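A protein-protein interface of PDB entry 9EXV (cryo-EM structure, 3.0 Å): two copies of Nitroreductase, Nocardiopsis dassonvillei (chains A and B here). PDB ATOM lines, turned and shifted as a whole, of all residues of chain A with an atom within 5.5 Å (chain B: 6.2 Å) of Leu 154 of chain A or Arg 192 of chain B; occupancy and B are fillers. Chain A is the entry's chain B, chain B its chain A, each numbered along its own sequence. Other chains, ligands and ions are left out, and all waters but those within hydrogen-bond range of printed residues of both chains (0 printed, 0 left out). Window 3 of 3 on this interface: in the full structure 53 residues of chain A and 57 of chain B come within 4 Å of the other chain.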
ATOM      1  N   VAL A  66       8.600  30.156 -14.595  1.00  0.00           N
ATOM      2  CA  VAL A  66       9.467  29.147 -15.192  1.00  0.00           C
ATOM      3  C   VAL A  66       9.039  28.960 -16.640  1.00  0.00           C
ATOM      4  O   VAL A  66       7.844  28.830 -16.924  1.00  0.00           O
ATOM      5  CB  VAL A  66       9.403  27.810 -14.427  1.00  0.00           C
ATOM      6  CG1 VAL A  66      10.205  26.742 -15.153  1.00  0.00           C
ATOM      7  CG2 VAL A  66       9.907  27.984 -13.002  1.00  0.00           C
ATOM      8  N   VAL A  68       9.388  26.531 -19.478  1.00  0.00           N
ATOM      9  CA  VAL A  68       9.739  25.189 -19.927  1.00  0.00           C
ATOM     10  C   VAL A  68       9.622  25.121 -21.443  1.00  0.00           C
ATOM     11  O   VAL A  68       8.571  25.438 -22.012  1.00  0.00           O
ATOM     12  CB  VAL A  68       8.837  24.140 -19.256  1.00  0.00           C
ATOM     13  CG1 VAL A  68       8.980  22.794 -19.944  1.00  0.00           C
ATOM     14  CG2 VAL A  68       9.166  24.025 -17.777  1.00  0.00           C
ATOM     15  N   ALA A  73      10.481  17.708 -20.776  1.00  0.00           N
ATOM     16  CA  ALA A  73       9.812  18.427 -19.699  1.00  0.00           C
ATOM     17  C   ALA A  73       8.394  18.811 -20.097  1.00  0.00           C
ATOM     18  O   ALA A  73       7.471  18.749 -19.277  1.00  0.00           O
ATOM     19  CB  ALA A  73      10.618  19.664 -19.312  1.00  0.00           C
ATOM     20  N   LEU A  76       6.237  15.682 -19.834  1.00  0.00           N
ATOM     21  CA  LEU A  76       5.990  15.349 -18.436  1.00  0.00           C
ATOM     22  C   LEU A  76       4.972  16.297 -17.814  1.00  0.00           C
ATOM     23  O   LEU A  76       4.059  15.861 -17.102  1.00  0.00           O
ATOM     24  CB  LEU A  76       7.298  15.367 -17.646  1.00  0.00           C
ATOM     25  CG  LEU A  76       7.958  13.995 -17.497  1.00  0.00           C
ATOM     26  CD1 LEU A  76       8.280  13.401 -18.859  1.00  0.00           C
ATOM     27  CD2 LEU A  76       9.206  14.075 -16.633  1.00  0.00           C
ATOM     28  N   LEU A  77       5.108  17.597 -18.075  1.00  0.00           N
ATOM     29  CA  LEU A  77       4.164  18.566 -17.529  1.00  0.00           C
ATOM     30  C   LEU A  77       2.763  18.343 -18.080  1.00  0.00           C
ATOM     31  O   LEU A  77       1.778  18.441 -17.344  1.00  0.00           O
ATOM     32  CB  LEU A  77       4.642  19.985 -17.816  1.00  0.00           C
ATOM     33  CG  LEU A  77       5.655  20.522 -16.804  1.00  0.00           C
ATOM     34  CD1 LEU A  77       6.415  21.703 -17.370  1.00  0.00           C
ATOM     35  CD2 LEU A  77       4.950  20.910 -15.514  1.00  0.00           C
ATOM     36  N   PHE A  80       1.274  15.411 -16.304  1.00  0.00           N
ATOM     37  CA  PHE A  80       0.940  15.712 -14.922  1.00  0.00           C
ATOM     38  C   PHE A  80       0.065  16.948 -14.765  1.00  0.00           C
ATOM     39  O   PHE A  80      -0.200  17.364 -13.635  1.00  0.00           O
ATOM     40  CB  PHE A  80       2.213  15.857 -14.091  1.00  0.00           C
ATOM     41  CG  PHE A  80       2.768  14.549 -13.649  1.00  0.00           C
ATOM     42  CD1 PHE A  80       2.030  13.745 -12.801  1.00  0.00           C
ATOM     43  CD2 PHE A  80       3.995  14.102 -14.098  1.00  0.00           C
ATOM     44  CE1 PHE A  80       2.508  12.533 -12.396  1.00  0.00           C
ATOM     45  CE2 PHE A  80       4.478  12.885 -13.690  1.00  0.00           C
ATOM     46  CZ  PHE A  80       3.721  12.104 -12.851  1.00  0.00           C
ATOM     47  N   GLY A 149       1.892  18.762  -6.505  1.00  0.00           N
ATOM     48  CA  GLY A 149       3.037  18.008  -6.048  1.00  0.00           C
ATOM     49  C   GLY A 149       3.964  17.595  -7.173  1.00  0.00           C
ATOM     50  O   GLY A 149       5.113  18.039  -7.257  1.00  0.00           O
ATOM     51  N   PRO A 150       3.481  16.714  -8.053  1.00  0.00           N
ATOM     52  CA  PRO A 150       4.331  16.270  -9.170  1.00  0.00           C
ATOM     53  C   PRO A 150       4.793  17.406 -10.067  1.00  0.00           C
ATOM     54  O   PRO A 150       5.940  17.390 -10.527  1.00  0.00           O
ATOM     55  CB  PRO A 150       3.428  15.280  -9.920  1.00  0.00           C
ATOM     56  CG  PRO A 150       2.432  14.824  -8.904  1.00  0.00           C
ATOM     57  CD  PRO A 150       2.191  16.004  -8.017  1.00  0.00           C
ATOM     58  N   VAL A 151       3.938  18.399 -10.318  1.00  0.00           N
ATOM     59  CA  VAL A 151       4.333  19.519 -11.171  1.00  0.00           C
ATOM     60  C   VAL A 151       5.469  20.303 -10.530  1.00  0.00           C
ATOM     61  O   VAL A 151       6.441  20.679 -11.195  1.00  0.00           O
ATOM     62  CB  VAL A 151       3.116  20.413 -11.472  1.00  0.00           C
ATOM     63  CG1 VAL A 151       3.558  21.784 -11.948  1.00  0.00           C
ATOM     64  CG2 VAL A 151       2.221  19.750 -12.508  1.00  0.00           C
ATOM     65  N   ARG A 152       5.360  20.561  -9.225  1.00  0.00           N
ATOM     66  CA  ARG A 152       6.453  21.185  -8.489  1.00  0.00           C
ATOM     67  C   ARG A 152       7.727  20.363  -8.610  1.00  0.00           C
ATOM     68  O   ARG A 152       8.811  20.903  -8.850  1.00  0.00           O
ATOM     69  CB  ARG A 152       6.057  21.342  -7.019  1.00  0.00           C
ATOM     70  CG  ARG A 152       7.209  21.379  -6.024  1.00  0.00           C
ATOM     71  CD  ARG A 152       6.695  21.171  -4.610  1.00  0.00           C
ATOM     72  NE  ARG A 152       5.612  22.094  -4.302  1.00  0.00           N
ATOM     73  CZ  ARG A 152       5.787  23.381  -4.045  1.00  0.00           C
ATOM     74  NH1 ARG A 152       6.991  23.928  -4.048  1.00  0.00           N
ATOM     75  NH2 ARG A 152       4.728  24.141  -3.781  1.00  0.00           N
ATOM     76  N   ARG A 153       7.609  19.045  -8.451  1.00  0.00           N
ATOM     77  CA  ARG A 153       8.786  18.193  -8.502  1.00  0.00           C
ATOM     78  C   ARG A 153       9.468  18.274  -9.859  1.00  0.00           C
ATOM     79  O   ARG A 153      10.701  18.349  -9.938  1.00  0.00           O
ATOM     80  CB  ARG A 153       8.397  16.760  -8.173  1.00  0.00           C
ATOM     81  CG  ARG A 153       7.919  16.554  -6.742  1.00  0.00           C
ATOM     82  CD  ARG A 153       7.533  15.111  -6.473  1.00  0.00           C
ATOM     83  NE  ARG A 153       8.679  14.216  -6.580  1.00  0.00           N
ATOM     84  CZ  ARG A 153       9.093  13.653  -7.708  1.00  0.00           C
ATOM     85  NH1 ARG A 153       8.450  13.835  -8.852  1.00  0.00           N
ATOM     86  NH2 ARG A 153      10.185  12.897  -7.692  1.00  0.00           N
ATOM     87  N   LEU A 154       8.687  18.264 -10.942  1.00  0.00           N
ATOM     88  CA  LEU A 154       9.274  18.407 -12.269  1.00  0.00           C
ATOM     89  C   LEU A 154       9.913  19.777 -12.448  1.00  0.00           C
ATOM     90  O   LEU A 154      11.014  19.888 -12.995  1.00  0.00           O
ATOM     91  CB  LEU A 154       8.215  18.170 -13.346  1.00  0.00           C
ATOM     92  CG  LEU A 154       7.380  16.896 -13.224  1.00  0.00           C
ATOM     93  CD1 LEU A 154       6.334  16.831 -14.326  1.00  0.00           C
ATOM     94  CD2 LEU A 154       8.257  15.652 -13.221  1.00  0.00           C
ATOM     95  N   LEU A 155       9.237  20.831 -11.988  1.00  0.00           N
ATOM     96  CA  LEU A 155       9.758  22.184 -12.138  1.00  0.00           C
ATOM     97  C   LEU A 155      10.939  22.461 -11.218  1.00  0.00           C
ATOM     98  O   LEU A 155      11.674  23.427 -11.450  1.00  0.00           O
ATOM     99  CB  LEU A 155       8.647  23.202 -11.883  1.00  0.00           C
ATOM    100  CG  LEU A 155       7.519  23.208 -12.915  1.00  0.00           C
ATOM    101  CD1 LEU A 155       6.278  23.886 -12.361  1.00  0.00           C
ATOM    102  CD2 LEU A 155       7.974  23.894 -14.192  1.00  0.00           C
ATOM    103  N   GLY A 156      11.141  21.643 -10.187  1.00  0.00           N
ATOM    104  CA  GLY A 156      12.221  21.880  -9.253  1.00  0.00           C
ATOM    105  C   GLY A 156      12.037  23.097  -8.377  1.00  0.00           C
ATOM    106  O   GLY A 156      13.023  23.650  -7.885  1.00  0.00           O
ATOM    107  N   SER B 189      13.041  31.879 -15.058  1.00  0.00           N
ATOM    108  CA  SER B 189      14.053  30.854 -15.257  1.00  0.00           C
ATOM    109  C   SER B 189      13.678  30.024 -16.475  1.00  0.00           C
ATOM    110  O   SER B 189      12.585  30.160 -17.032  1.00  0.00           O
ATOM    111  CB  SER B 189      14.199  29.976 -14.012  1.00  0.00           C
ATOM    112  OG  SER B 189      12.944  29.439 -13.632  1.00  0.00           O
ATOM    113  N   HIS B 190      14.599  29.158 -16.892  1.00  0.00           N
ATOM    114  CA  HIS B 190      14.436  28.343 -18.094  1.00  0.00           C
ATOM    115  C   HIS B 190      14.290  26.878 -17.694  1.00  0.00           C
ATOM    116  O   HIS B 190      15.274  26.223 -17.338  1.00  0.00           O
ATOM    117  CB  HIS B 190      15.607  28.557 -19.048  1.00  0.00           C
ATOM    118  CG  HIS B 190      15.576  29.885 -19.738  1.00  0.00           C
ATOM    119  ND1 HIS B 190      14.453  30.685 -19.755  1.00  0.00           N
ATOM    120  CD2 HIS B 190      16.526  30.557 -20.432  1.00  0.00           C
ATOM    121  CE1 HIS B 190      14.711  31.790 -20.431  1.00  0.00           C
ATOM    122  NE2 HIS B 190      15.963  31.738 -20.852  1.00  0.00           N
ATOM    123  N   GLU B 191      13.049  26.385 -17.733  1.00  0.00           N
ATOM    124  CA  GLU B 191      12.652  24.992 -17.542  1.00  0.00           C
ATOM    125  C   GLU B 191      13.111  24.403 -16.214  1.00  0.00           C
ATOM    126  O   GLU B 191      12.933  23.200 -15.986  1.00  0.00           O
ATOM    127  CB  GLU B 191      13.118  24.092 -18.700  1.00  0.00           C
ATOM    128  CG  GLU B 191      14.619  23.846 -18.808  1.00  0.00           C
ATOM    129  CD  GLU B 191      15.275  24.692 -19.889  1.00  0.00           C
ATOM    130  OE1 GLU B 191      14.653  25.673 -20.347  1.00  0.00           O
ATOM    131  OE2 GLU B 191      16.412  24.364 -20.287  1.00  0.00           O
ATOM    132  N   ARG B 192      13.664  25.213 -15.323  1.00  0.00           N
ATOM    133  CA  ARG B 192      14.155  24.755 -14.029  1.00  0.00           C
ATOM    134  C   ARG B 192      14.131  25.948 -13.082  1.00  0.00           C
ATOM    135  O   ARG B 192      13.516  26.977 -13.376  1.00  0.00           O
ATOM    136  CB  ARG B 192      15.550  24.135 -14.156  1.00  0.00           C
ATOM    137  CG  ARG B 192      15.589  22.730 -14.758  1.00  0.00           C
ATOM    138  CD  ARG B 192      14.927  21.710 -13.843  1.00  0.00           C
ATOM    139  NE  ARG B 192      15.608  21.634 -12.556  1.00  0.00           N
ATOM    140  CZ  ARG B 192      15.243  20.846 -11.555  1.00  0.00           C
ATOM    141  NH1 ARG B 192      14.197  20.041 -11.652  1.00  0.00           N
ATOM    142  NH2 ARG B 192      15.946  20.866 -10.425  1.00  0.00           N
ATOM    143  N   TRP B 193      14.790  25.814 -11.937  1.00  0.00           N
ATOM    144  CA  TRP B 193      14.970  26.920 -11.008  1.00  0.00           C
ATOM    145  C   TRP B 193      16.457  27.185 -10.840  1.00  0.00           C
ATOM    146  O   TRP B 193      17.228  26.262 -10.550  1.00  0.00           O
ATOM    147  CB  TRP B 193      14.317  26.630  -9.655  1.00  0.00           C
ATOM    148  CG  TRP B 193      14.097  27.860  -8.826  1.00  0.00           C
ATOM    149  CD1 TRP B 193      14.516  28.075  -7.549  1.00  0.00           C
ATOM    150  CD2 TRP B 193      13.414  29.055  -9.229  1.00  0.00           C
ATOM    151  NE1 TRP B 193      14.125  29.321  -7.122  1.00  0.00           N
ATOM    152  CE2 TRP B 193      13.451  29.945  -8.138  1.00  0.00           C
ATOM    153  CE3 TRP B 193      12.773  29.459 -10.406  1.00  0.00           C
ATOM    154  CZ2 TRP B 193      12.876  31.213  -8.190  1.00  0.00           C
ATOM    155  CZ3 TRP B 193      12.201  30.715 -10.454  1.00  0.00           C
ATOM    156  CH2 TRP B 193      12.254  31.577  -9.353  1.00  0.00           C
ATOM    157  N   GLY B 194      16.856  28.442 -11.023  1.00  0.00           N
ATOM    158  CA  GLY B 194      18.246  28.827 -10.930  1.00  0.00           C
ATOM    159  C   GLY B 194      19.062  28.611 -12.183  1.00  0.00           C
ATOM    160  O   GLY B 194      20.263  28.910 -12.178  1.00  0.00           O
ATOM    161  N   THR B 195      18.460  28.106 -13.255  1.00  0.00           N
ATOM    162  CA  THR B 195      19.175  27.882 -14.506  1.00  0.00           C
ATOM    163  C   THR B 195      18.879  28.995 -15.505  1.00  0.00           C
ATOM    164  O   THR B 195      19.783  29.511 -16.161  1.00  0.00           O
ATOM    165  CB  THR B 195      18.809  26.526 -15.138  1.00  0.00           C
ATOM    166  OG1 THR B 195      17.414  26.513 -15.469  1.00  0.00           O
ATOM    167  CG2 THR B 195      19.109  25.387 -14.174  1.00  0.00           C
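Of the 7 printed residues of chain B, 4 touch a printed residue of chain A.
Printed residues of chain B that touch a printed residue of chain A: Ser 189, Glu 191, Arg 192 and Trp 193.
Among the printed residues, 9 pairs touch across the chains.
Among the printed residues, merely in contact across the chains: Val 66 of chain A with Ser 189 of chain B (3.4 Å), Gly 156 of chain A with Arg 192 of chain B (3.6 Å), Val 68 of chain A with Glu 191 of chain B (3.6 Å), Gly 156 of chain A with Trp 193 of chain B (3.7 Å), Val 66 of chain A with Arg 192 of chain B (3.8 Å), Leu 155 of chain A with Arg 192 of chain B (3.8 Å), Val 66 of chain A with Glu 191 of chain B (3.8 Å) and Leu 155 of chain A with Trp 193 of chain B (3.96 Å).
No position is printed for both chains.
Ala 73 of chain A touches none of the printed residues of chain B.
Leu 76 of chain A touches none of the printed residues of chain B.
Of chain B, only Arg 192 comes within 4 Å of Leu 154 of chain A.
Printed residues of chain B within 4 Å of Gly 156 of chain A: Arg 192 (3.6 Å) and Trp 193 (3.7 Å).
Of the printed residues of chain A, Ser 189 of chain B touches Val 66 (3.4 Å).
Printed residues of chain A within 4 Å of Glu 191 of chain B: Val 66 and Val 68.
Printed residues of chain A within 4 Å of Trp 193 of chain B: Leu 155 (3.96 Å) and Gly 156 (3.7 Å).
The nearest residue of chain A that does not touch Arg 192 of chain B is Arg 153 of chain A (4.2 Å).
The nearest printed residue of chain A that does not touch Glu 191 of chain B is Leu 155 of chain A (4.7 Å).
The backbone carbonyl oxygen of Arg 192 of chain B is in hydrogen-bond range of the side-chain hydroxyl of Ser 189 of chain B, at 2.5 Å.
O of Leu 154 of chain A is in hydrogen-bond range of NH1 of Arg 192 of chain B (3.5 Å).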
